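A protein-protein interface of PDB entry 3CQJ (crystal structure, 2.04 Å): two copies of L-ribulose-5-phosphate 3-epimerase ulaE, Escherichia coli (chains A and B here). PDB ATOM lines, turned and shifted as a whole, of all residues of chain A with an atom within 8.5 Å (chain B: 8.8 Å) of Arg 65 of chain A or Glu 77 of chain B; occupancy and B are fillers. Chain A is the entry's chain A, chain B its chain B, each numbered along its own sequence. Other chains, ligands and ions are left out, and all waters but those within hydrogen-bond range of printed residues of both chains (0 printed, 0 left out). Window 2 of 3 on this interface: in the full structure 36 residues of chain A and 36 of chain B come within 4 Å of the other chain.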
ATOM      1  N   ASP A  62      -9.050 -12.081  13.342  1.00  0.00           N
ATOM      2  CA  ASP A  62     -10.040 -11.041  13.052  1.00  0.00           C
ATOM      3  C   ASP A  62     -11.190 -11.551  12.193  1.00  0.00           C
ATOM      4  O   ASP A  62     -11.998 -10.756  11.708  1.00  0.00           O
ATOM      5  CB  ASP A  62      -9.376  -9.829  12.398  1.00  0.00           C
ATOM      6  CG  ASP A  62      -8.272  -9.254  13.246  1.00  0.00           C
ATOM      7  OD1 ASP A  62      -8.479  -9.086  14.475  1.00  0.00           O
ATOM      8  OD2 ASP A  62      -7.184  -9.000  12.681  1.00  0.00           O
ATOM      9  N   TRP A  63     -11.261 -12.875  12.007  1.00  0.00           N
ATOM     10  CA  TRP A  63     -12.357 -13.510  11.272  1.00  0.00           C
ATOM     11  C   TRP A  63     -13.723 -13.062  11.794  1.00  0.00           C
ATOM     12  O   TRP A  63     -13.912 -12.873  13.001  1.00  0.00           O
ATOM     13  CB  TRP A  63     -12.278 -15.032  11.392  1.00  0.00           C
ATOM     14  CG  TRP A  63     -11.475 -15.760  10.349  1.00  0.00           C
ATOM     15  CD1 TRP A  63     -10.684 -15.227   9.376  1.00  0.00           C
ATOM     16  CD2 TRP A  63     -11.370 -17.186  10.217  1.00  0.00           C
ATOM     17  NE1 TRP A  63     -10.105 -16.233   8.632  1.00  0.00           N
ATOM     18  CE2 TRP A  63     -10.513 -17.444   9.128  1.00  0.00           C
ATOM     19  CE3 TRP A  63     -11.935 -18.271  10.909  1.00  0.00           C
ATOM     20  CZ2 TRP A  63     -10.211 -18.745   8.702  1.00  0.00           C
ATOM     21  CZ3 TRP A  63     -11.618 -19.574  10.495  1.00  0.00           C
ATOM     22  CH2 TRP A  63     -10.767 -19.791   9.400  1.00  0.00           C
ATOM     23  N   SER A  64     -14.669 -12.904  10.873  1.00  0.00           N
ATOM     24  CA  SER A  64     -16.064 -12.655  11.221  1.00  0.00           C
ATOM     25  C   SER A  64     -16.701 -13.892  11.858  1.00  0.00           C
ATOM     26  O   SER A  64     -16.177 -15.007  11.738  1.00  0.00           O
ATOM     27  CB  SER A  64     -16.862 -12.281   9.966  1.00  0.00           C
ATOM     28  OG  SER A  64     -17.086 -13.419   9.147  1.00  0.00           O
ATOM     29  N   ARG A  65     -17.853 -13.687  12.496  1.00  0.00           N
ATOM     30  CA  ARG A  65     -18.650 -14.776  13.062  1.00  0.00           C
ATOM     31  C   ARG A  65     -18.966 -15.829  12.003  1.00  0.00           C
ATOM     32  O   ARG A  65     -18.797 -17.028  12.236  1.00  0.00           O
ATOM     33  CB  ARG A  65     -19.932 -14.211  13.704  1.00  0.00           C
ATOM     34  CG  ARG A  65     -19.643 -13.442  14.997  1.00  0.00           C
ATOM     35  CD  ARG A  65     -20.897 -12.826  15.627  1.00  0.00           C
ATOM     36  NE  ARG A  65     -21.291 -11.587  14.962  1.00  0.00           N
ATOM     37  CZ  ARG A  65     -22.385 -10.894  15.255  1.00  0.00           C
ATOM     38  NH1 ARG A  65     -23.219 -11.329  16.206  1.00  0.00           N
ATOM     39  NH2 ARG A  65     -22.656  -9.774  14.584  1.00  0.00           N
ATOM     40  N   GLU A  66     -19.372 -15.380  10.819  1.00  0.00           N
ATOM     41  CA  GLU A  66     -19.643 -16.303   9.711  1.00  0.00           C
ATOM     42  C   GLU A  66     -18.418 -17.109   9.280  1.00  0.00           C
ATOM     43  O   GLU A  66     -18.546 -18.274   8.937  1.00  0.00           O
ATOM     44  CB  GLU A  66     -20.267 -15.586   8.508  1.00  0.00           C
ATOM     45  CG  GLU A  66     -21.710 -15.100   8.728  1.00  0.00           C
ATOM     46  CD  GLU A  66     -21.805 -13.823   9.572  1.00  0.00           C
ATOM     47  OE1 GLU A  66     -20.814 -13.060   9.639  1.00  0.00           O
ATOM     48  OE2 GLU A  66     -22.882 -13.581  10.170  1.00  0.00           O
ATOM     49  N   GLN A  67     -17.237 -16.499   9.290  1.00  0.00           N
ATOM     50  CA  GLN A  67     -16.005 -17.244   8.989  1.00  0.00           C
ATOM     51  C   GLN A  67     -15.692 -18.290  10.075  1.00  0.00           C
ATOM     52  O   GLN A  67     -15.356 -19.441   9.765  1.00  0.00           O
ATOM     53  CB  GLN A  67     -14.814 -16.307   8.786  1.00  0.00           C
ATOM     54  CG  GLN A  67     -14.906 -15.481   7.488  1.00  0.00           C
ATOM     55  CD  GLN A  67     -13.778 -14.484   7.366  1.00  0.00           C
ATOM     56  OE1 GLN A  67     -13.625 -13.601   8.208  1.00  0.00           O
ATOM     57  NE2 GLN A  67     -12.980 -14.617   6.315  1.00  0.00           N
ATOM     58  N   ARG A  68     -15.822 -17.885  11.335  1.00  0.00           N
ATOM     59  CA  ARG A  68     -15.620 -18.801  12.475  1.00  0.00           C
ATOM     60  C   ARG A  68     -16.588 -19.977  12.396  1.00  0.00           C
ATOM     61  O   ARG A  68     -16.189 -21.138  12.523  1.00  0.00           O
ATOM     62  CB  ARG A  68     -15.769 -18.042  13.802  1.00  0.00           C
ATOM     63  CG  ARG A  68     -14.626 -17.048  14.048  1.00  0.00           C
ATOM     64  CD  ARG A  68     -14.974 -15.947  15.054  1.00  0.00           C
ATOM     65  NE  ARG A  68     -14.037 -14.833  14.906  1.00  0.00           N
ATOM     66  CZ  ARG A  68     -13.076 -14.522  15.768  1.00  0.00           C
ATOM     67  NH1 ARG A  68     -12.927 -15.208  16.900  1.00  0.00           N
ATOM     68  NH2 ARG A  68     -12.263 -13.506  15.500  1.00  0.00           N
ATOM     69  N   LEU A  69     -17.850 -19.673  12.109  1.00  0.00           N
ATOM     70  CA  LEU A  69     -18.898 -20.674  12.064  1.00  0.00           C
ATOM     71  C   LEU A  69     -18.783 -21.596  10.860  1.00  0.00           C
ATOM     72  O   LEU A  69     -19.181 -22.757  10.947  1.00  0.00           O
ATOM     73  CB  LEU A  69     -20.281 -20.024  12.152  1.00  0.00           C
ATOM     74  CG  LEU A  69     -20.588 -19.394  13.521  1.00  0.00           C
ATOM     75  CD1 LEU A  69     -21.901 -18.614  13.527  1.00  0.00           C
ATOM     76  CD2 LEU A  69     -20.583 -20.465  14.640  1.00  0.00           C
ATOM     77  N   ALA A  70     -18.238 -21.088   9.753  1.00  0.00           N
ATOM     78  CA  ALA A  70     -17.935 -21.922   8.583  1.00  0.00           C
ATOM     79  C   ALA A  70     -16.867 -22.962   8.906  1.00  0.00           C
ATOM     80  O   ALA A  70     -16.940 -24.093   8.434  1.00  0.00           O
ATOM     81  CB  ALA A  70     -17.481 -21.074   7.405  1.00  0.00           C
ATOM     82  N   LEU A  71     -15.851 -22.571   9.671  1.00  0.00           N
ATOM     83  CA  LEU A  71     -14.876 -23.562  10.142  1.00  0.00           C
ATOM     84  C   LEU A  71     -15.558 -24.657  10.986  1.00  0.00           C
ATOM     85  O   LEU A  71     -15.348 -25.840  10.740  1.00  0.00           O
ATOM     86  CB  LEU A  71     -13.720 -22.909  10.901  1.00  0.00           C
ATOM     87  CG  LEU A  71     -12.641 -23.842  11.474  1.00  0.00           C
ATOM     88  CD1 LEU A  71     -11.983 -24.721  10.394  1.00  0.00           C
ATOM     89  CD2 LEU A  71     -11.604 -23.013  12.240  1.00  0.00           C
ATOM     90  N   VAL A  72     -16.387 -24.260  11.953  1.00  0.00           N
ATOM     91  CA  VAL A  72     -17.109 -25.228  12.798  1.00  0.00           C
ATOM     92  C   VAL A  72     -17.943 -26.177  11.932  1.00  0.00           C
ATOM     93  O   VAL A  72     -17.919 -27.399  12.124  1.00  0.00           O
ATOM     94  CB  VAL A  72     -17.992 -24.519  13.875  1.00  0.00           C
ATOM     95  CG1 VAL A  72     -18.745 -25.539  14.737  1.00  0.00           C
ATOM     96  CG2 VAL A  72     -17.142 -23.633  14.762  1.00  0.00           C
ATOM     97  N   GLN A 115     -10.203 -16.210  22.564  1.00  0.00           N
ATOM     98  CA  GLN A 115     -11.573 -15.992  22.068  1.00  0.00           C
ATOM     99  C   GLN A 115     -11.864 -16.841  20.820  1.00  0.00           C
ATOM    100  O   GLN A 115     -12.937 -17.435  20.713  1.00  0.00           O
ATOM    101  CB  GLN A 115     -11.846 -14.507  21.784  1.00  0.00           C
ATOM    102  CG  GLN A 115     -13.330 -14.214  21.493  1.00  0.00           C
ATOM    103  CD  GLN A 115     -13.661 -12.728  21.426  1.00  0.00           C
ATOM    104  OE1 GLN A 115     -12.790 -11.870  21.613  1.00  0.00           O
ATOM    105  NE2 GLN A 115     -14.930 -12.416  21.158  1.00  0.00           N
ATOM    106  N   ASP A 119     -14.597 -19.792  20.226  1.00  0.00           N
ATOM    107  CA  ASP A 119     -15.550 -19.734  19.114  1.00  0.00           C
ATOM    108  C   ASP A 119     -15.618 -21.011  18.271  1.00  0.00           C
ATOM    109  O   ASP A 119     -16.705 -21.501  17.961  1.00  0.00           O
ATOM    110  CB  ASP A 119     -15.202 -18.553  18.206  1.00  0.00           C
ATOM    111  CG  ASP A 119     -15.588 -17.204  18.814  1.00  0.00           C
ATOM    112  OD1 ASP A 119     -16.406 -17.178  19.758  1.00  0.00           O
ATOM    113  OD2 ASP A 119     -15.063 -16.166  18.346  1.00  0.00           O
ATOM    114  N   VAL A 120     -14.457 -21.531  17.884  1.00  0.00           N
ATOM    115  CA  VAL A 120     -14.413 -22.676  16.983  1.00  0.00           C
ATOM    116  C   VAL A 120     -14.185 -24.016  17.706  1.00  0.00           C
ATOM    117  O   VAL A 120     -14.128 -25.063  17.066  1.00  0.00           O
ATOM    118  CB  VAL A 120     -13.394 -22.472  15.830  1.00  0.00           C
ATOM    119  CG1 VAL A 120     -13.729 -21.203  15.049  1.00  0.00           C
ATOM    120  CG2 VAL A 120     -11.987 -22.398  16.362  1.00  0.00           C
ATOM    121  N   LEU B  33     -31.373 -20.150  21.892  1.00  0.00           N
ATOM    122  CA  LEU B  33     -31.172 -18.724  21.584  1.00  0.00           C
ATOM    123  C   LEU B  33     -31.888 -17.823  22.599  1.00  0.00           C
ATOM    124  O   LEU B  33     -31.301 -16.872  23.111  1.00  0.00           O
ATOM    125  CB  LEU B  33     -31.603 -18.385  20.148  1.00  0.00           C
ATOM    126  CG  LEU B  33     -31.485 -16.935  19.647  1.00  0.00           C
ATOM    127  CD1 LEU B  33     -30.044 -16.449  19.616  1.00  0.00           C
ATOM    128  CD2 LEU B  33     -32.120 -16.793  18.264  1.00  0.00           C
ATOM    129  N   GLU B  34     -33.146 -18.155  22.887  1.00  0.00           N
ATOM    130  CA  GLU B  34     -33.974 -17.440  23.859  1.00  0.00           C
ATOM    131  C   GLU B  34     -33.371 -17.486  25.273  1.00  0.00           C
ATOM    132  O   GLU B  34     -33.303 -16.465  25.965  1.00  0.00           O
ATOM    133  CB  GLU B  34     -35.388 -18.041  23.852  1.00  0.00           C
ATOM    134  CG  GLU B  34     -36.460 -17.207  24.523  1.00  0.00           C
ATOM    135  CD  GLU B  34     -37.866 -17.824  24.409  1.00  0.00           C
ATOM    136  OE1 GLU B  34     -38.037 -19.039  24.696  1.00  0.00           O
ATOM    137  OE2 GLU B  34     -38.807 -17.083  24.044  1.00  0.00           O
ATOM    138  N   LEU B  36     -30.159 -18.123  26.080  1.00  0.00           N
ATOM    139  CA  LEU B  36     -28.873 -17.413  26.088  1.00  0.00           C
ATOM    140  C   LEU B  36     -29.067 -15.887  26.093  1.00  0.00           C
ATOM    141  O   LEU B  36     -28.370 -15.159  26.819  1.00  0.00           O
ATOM    142  CB  LEU B  36     -27.985 -17.865  24.917  1.00  0.00           C
ATOM    143  CG  LEU B  36     -27.438 -19.305  24.928  1.00  0.00           C
ATOM    144  CD1 LEU B  36     -26.745 -19.635  23.607  1.00  0.00           C
ATOM    145  CD2 LEU B  36     -26.497 -19.584  26.119  1.00  0.00           C
ATOM    146  N   GLN B  37     -30.031 -15.416  25.299  1.00  0.00           N
ATOM    147  CA  GLN B  37     -30.429 -13.997  25.312  1.00  0.00           C
ATOM    148  C   GLN B  37     -30.965 -13.557  26.679  1.00  0.00           C
ATOM    149  O   GLN B  37     -30.650 -12.461  27.139  1.00  0.00           O
ATOM    150  CB  GLN B  37     -31.451 -13.698  24.207  1.00  0.00           C
ATOM    151  CG  GLN B  37     -30.834 -13.612  22.815  1.00  0.00           C
ATOM    152  CD  GLN B  37     -31.870 -13.522  21.701  1.00  0.00           C
ATOM    153  OE1 GLN B  37     -32.975 -14.069  21.808  1.00  0.00           O
ATOM    154  NE2 GLN B  37     -31.509 -12.842  20.610  1.00  0.00           N
ATOM    155  N   LYS B  40     -28.010 -13.154  28.998  1.00  0.00           N
ATOM    156  CA  LYS B  40     -27.309 -11.920  28.644  1.00  0.00           C
ATOM    157  C   LYS B  40     -27.959 -10.697  29.319  1.00  0.00           C
ATOM    158  O   LYS B  40     -27.271  -9.883  29.940  1.00  0.00           O
ATOM    159  CB  LYS B  40     -27.250 -11.744  27.118  1.00  0.00           C
ATOM    160  CG  LYS B  40     -26.279 -10.669  26.649  1.00  0.00           C
ATOM    161  CD  LYS B  40     -26.407 -10.406  25.152  1.00  0.00           C
ATOM    162  CE  LYS B  40     -25.158  -9.716  24.622  1.00  0.00           C
ATOM    163  NZ  LYS B  40     -25.238  -9.489  23.150  1.00  0.00           N
ATOM    164  N   ALA B  70     -26.768 -25.391  15.423  1.00  0.00           N
ATOM    165  CA  ALA B  70     -27.674 -24.317  15.844  1.00  0.00           C
ATOM    166  C   ALA B  70     -27.315 -23.788  17.233  1.00  0.00           C
ATOM    167  O   ALA B  70     -27.444 -22.588  17.495  1.00  0.00           O
ATOM    168  CB  ALA B  70     -29.129 -24.787  15.816  1.00  0.00           C
ATOM    169  N   LEU B  71     -26.865 -24.679  18.128  1.00  0.00           N
ATOM    170  CA  LEU B  71     -26.443 -24.235  19.453  1.00  0.00           C
ATOM    171  C   LEU B  71     -25.180 -23.385  19.353  1.00  0.00           C
ATOM    172  O   LEU B  71     -25.127 -22.284  19.903  1.00  0.00           O
ATOM    173  CB  LEU B  71     -26.255 -25.414  20.426  1.00  0.00           C
ATOM    174  CG  LEU B  71     -25.766 -25.075  21.840  1.00  0.00           C
ATOM    175  CD1 LEU B  71     -26.668 -24.023  22.537  1.00  0.00           C
ATOM    176  CD2 LEU B  71     -25.710 -26.354  22.670  1.00  0.00           C
ATOM    177  N   VAL B  72     -24.178 -23.897  18.645  1.00  0.00           N
ATOM    178  CA  VAL B  72     -22.955 -23.134  18.371  1.00  0.00           C
ATOM    179  C   VAL B  72     -23.262 -21.727  17.806  1.00  0.00           C
ATOM    180  O   VAL B  72     -22.745 -20.725  18.311  1.00  0.00           O
ATOM    181  CB  VAL B  72     -21.986 -23.918  17.449  1.00  0.00           C
ATOM    182  CG1 VAL B  72     -20.716 -23.094  17.154  1.00  0.00           C
ATOM    183  CG2 VAL B  72     -21.615 -25.276  18.090  1.00  0.00           C
ATOM    184  N   ASN B  73     -24.123 -21.666  16.784  1.00  0.00           N
ATOM    185  CA  ASN B  73     -24.544 -20.388  16.176  1.00  0.00           C
ATOM    186  C   ASN B  73     -25.111 -19.402  17.183  1.00  0.00           C
ATOM    187  O   ASN B  73     -24.727 -18.224  17.188  1.00  0.00           O
ATOM    188  CB  ASN B  73     -25.582 -20.619  15.069  1.00  0.00           C
ATOM    189  CG  ASN B  73     -25.013 -21.375  13.861  1.00  0.00           C
ATOM    190  OD1 ASN B  73     -23.809 -21.612  13.759  1.00  0.00           O
ATOM    191  ND2 ASN B  73     -25.895 -21.772  12.954  1.00  0.00           N
ATOM    192  N   ALA B  74     -26.008 -19.901  18.039  1.00  0.00           N
ATOM    193  CA  ALA B  74     -26.647 -19.103  19.087  1.00  0.00           C
ATOM    194  C   ALA B  74     -25.654 -18.577  20.129  1.00  0.00           C
ATOM    195  O   ALA B  74     -25.756 -17.428  20.557  1.00  0.00           O
ATOM    196  CB  ALA B  74     -27.751 -19.906  19.761  1.00  0.00           C
ATOM    197  N   ILE B  75     -24.706 -19.423  20.537  1.00  0.00           N
ATOM    198  CA  ILE B  75     -23.630 -19.019  21.442  1.00  0.00           C
ATOM    199  C   ILE B  75     -22.801 -17.892  20.819  1.00  0.00           C
ATOM    200  O   ILE B  75     -22.527 -16.879  21.456  1.00  0.00           O
ATOM    201  CB  ILE B  75     -22.707 -20.231  21.817  1.00  0.00           C
ATOM    202  CG1 ILE B  75     -23.466 -21.223  22.709  1.00  0.00           C
ATOM    203  CG2 ILE B  75     -21.417 -19.747  22.508  1.00  0.00           C
ATOM    204  CD1 ILE B  75     -22.896 -22.637  22.704  1.00  0.00           C
ATOM    205  N   VAL B  76     -22.412 -18.080  19.565  1.00  0.00           N
ATOM    206  CA  VAL B  76     -21.614 -17.085  18.864  1.00  0.00           C
ATOM    207  C   VAL B  76     -22.377 -15.760  18.638  1.00  0.00           C
ATOM    208  O   VAL B  76     -21.790 -14.689  18.769  1.00  0.00           O
ATOM    209  CB  VAL B  76     -20.984 -17.679  17.568  1.00  0.00           C
ATOM    210  CG1 VAL B  76     -20.363 -16.594  16.702  1.00  0.00           C
ATOM    211  CG2 VAL B  76     -19.930 -18.719  17.946  1.00  0.00           C
ATOM    212  N   GLU B  77     -23.679 -15.841  18.355  1.00  0.00           N
ATOM    213  CA  GLU B  77     -24.521 -14.647  18.139  1.00  0.00           C
ATOM    214  C   GLU B  77     -24.722 -13.824  19.414  1.00  0.00           C
ATOM    215  O   GLU B  77     -24.677 -12.594  19.369  1.00  0.00           O
ATOM    216  CB  GLU B  77     -25.894 -15.004  17.547  1.00  0.00           C
ATOM    217  CG  GLU B  77     -26.577 -13.808  16.810  1.00  0.00           C
ATOM    218  CD  GLU B  77     -28.086 -13.972  16.570  1.00  0.00           C
ATOM    219  OE1 GLU B  77     -28.547 -15.078  16.177  1.00  0.00           O
ATOM    220  OE2 GLU B  77     -28.821 -12.959  16.749  1.00  0.00           O
ATOM    221  N   THR B  78     -24.970 -14.504  20.535  1.00  0.00           N
ATOM    222  CA  THR B  78     -25.240 -13.840  21.815  1.00  0.00           C
ATOM    223  C   THR B  78     -23.955 -13.488  22.561  1.00  0.00           C
ATOM    224  O   THR B  78     -23.918 -12.529  23.323  1.00  0.00           O
ATOM    225  CB  THR B  78     -26.115 -14.718  22.737  1.00  0.00           C
ATOM    226  OG1 THR B  78     -25.482 -15.989  22.921  1.00  0.00           O
ATOM    227  CG2 THR B  78     -27.490 -14.938  22.128  1.00  0.00           C
ATOM    228  N   GLY B  79     -22.906 -14.276  22.348  1.00  0.00           N
ATOM    229  CA  GLY B  79     -21.671 -14.106  23.091  1.00  0.00           C
ATOM    230  C   GLY B  79     -21.785 -14.666  24.497  1.00  0.00           C
ATOM    231  O   GLY B  79     -20.902 -14.455  25.317  1.00  0.00           O
ATOM    232  N   VAL B  80     -22.891 -15.350  24.784  1.00  0.00           N
ATOM    233  CA  VAL B  80     -23.057 -16.084  26.036  1.00  0.00           C
ATOM    234  C   VAL B  80     -22.576 -17.518  25.800  1.00  0.00           C
ATOM    235  O   VAL B  80     -23.141 -18.232  24.980  1.00  0.00           O
ATOM    236  CB  VAL B  80     -24.536 -16.080  26.517  1.00  0.00           C
ATOM    237  CG1 VAL B  80     -24.678 -16.815  27.855  1.00  0.00           C
ATOM    238  CG2 VAL B  80     -25.069 -14.641  26.635  1.00  0.00           C
ATOM    239  N   ARG B  81     -21.530 -17.930  26.516  1.00  0.00           N
ATOM    240  CA  ARG B  81     -20.930 -19.245  26.303  1.00  0.00           C
ATOM    241  C   ARG B  81     -21.714 -20.371  26.992  1.00  0.00           C
ATOM    242  O   ARG B  81     -22.504 -20.122  27.909  1.00  0.00           O
ATOM    243  CB  ARG B  81     -19.460 -19.252  26.762  1.00  0.00           C
ATOM    244  CG  ARG B  81     -18.588 -18.107  26.209  1.00  0.00           C
ATOM    245  CD  ARG B  81     -18.287 -18.265  24.733  1.00  0.00           C
ATOM    246  NE  ARG B  81     -17.441 -17.187  24.205  1.00  0.00           N
ATOM    247  CZ  ARG B  81     -17.036 -17.104  22.938  1.00  0.00           C
ATOM    248  NH1 ARG B  81     -17.393 -18.037  22.055  1.00  0.00           N
ATOM    249  NH2 ARG B  81     -16.262 -16.089  22.549  1.00  0.00           N
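Among the printed residues, merely in contact across the chains: Arg 65 of chain A with Val 76 of chain B (3.7 Å), Arg 65 of chain A with Glu 77 of chain B (3.7 Å), Leu 69 of chain A with Val 72 of chain B (3.6 Å), Leu 69 of chain A with Asn 73 of chain B (3.5 Å), Leu 69 of chain A with Val 76 of chain B (3.8 Å), Val 72 of chain A with Val 72 of chain B (3.96 Å) and Gln 115 of chain A with Arg 81 of chain B (3.6 Å).
OD2 of Asp 119 of chain A lies within salt-bridge range of NH1 of Arg 68 of chain A.
Hydrophobic or aromatic side chains of chain A that line the printed part of chain B: Leu 69 and Val 72. Printed residues of chain B that touch a printed residue of chain A: Val 72, Asn 73, Val 76, Glu 77 and Arg 81. Among the printed residues, 8 pairs touch across the chains.
Val 72 of chain B touches its own counterpart, Val 72 of chain A. 3 positions are printed for both chains.
Of chain B, only Val 76 and Glu 77 come within 4 Å of Arg 65 of chain A. Glu 77 of chain B touches one residue of chain A. No residue of chain B comes within 4 Å of Ser 64 of chain A. No residue of chain B comes within 4 Å of Glu 66 of chain A. No residue of chain A comes within 4 Å of Thr 78 of chain B. Of the printed residues of chain B, Gln 115 of chain A touches Arg 81. Printed residues of chain B within 4 Å of Val 72 of chain A: Val 72. Of the printed residues of chain A, Asn 73 of chain B touches Leu 69. Printed residues of chain B within 4 Å of Asp 119 of chain A: Arg 81. The nearest residue of chain B that does not touch Arg 65 of chain A is Thr 78 of chain B (5.6 Å). The nearest residue of chain A that does not touch Glu 77 of chain B is Leu 69 of chain A (5.8 Å).
OD1 of Asp 119 of chain A is in salt-bridge range of NH1 of Arg 81 of chain B (2.6 Å).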
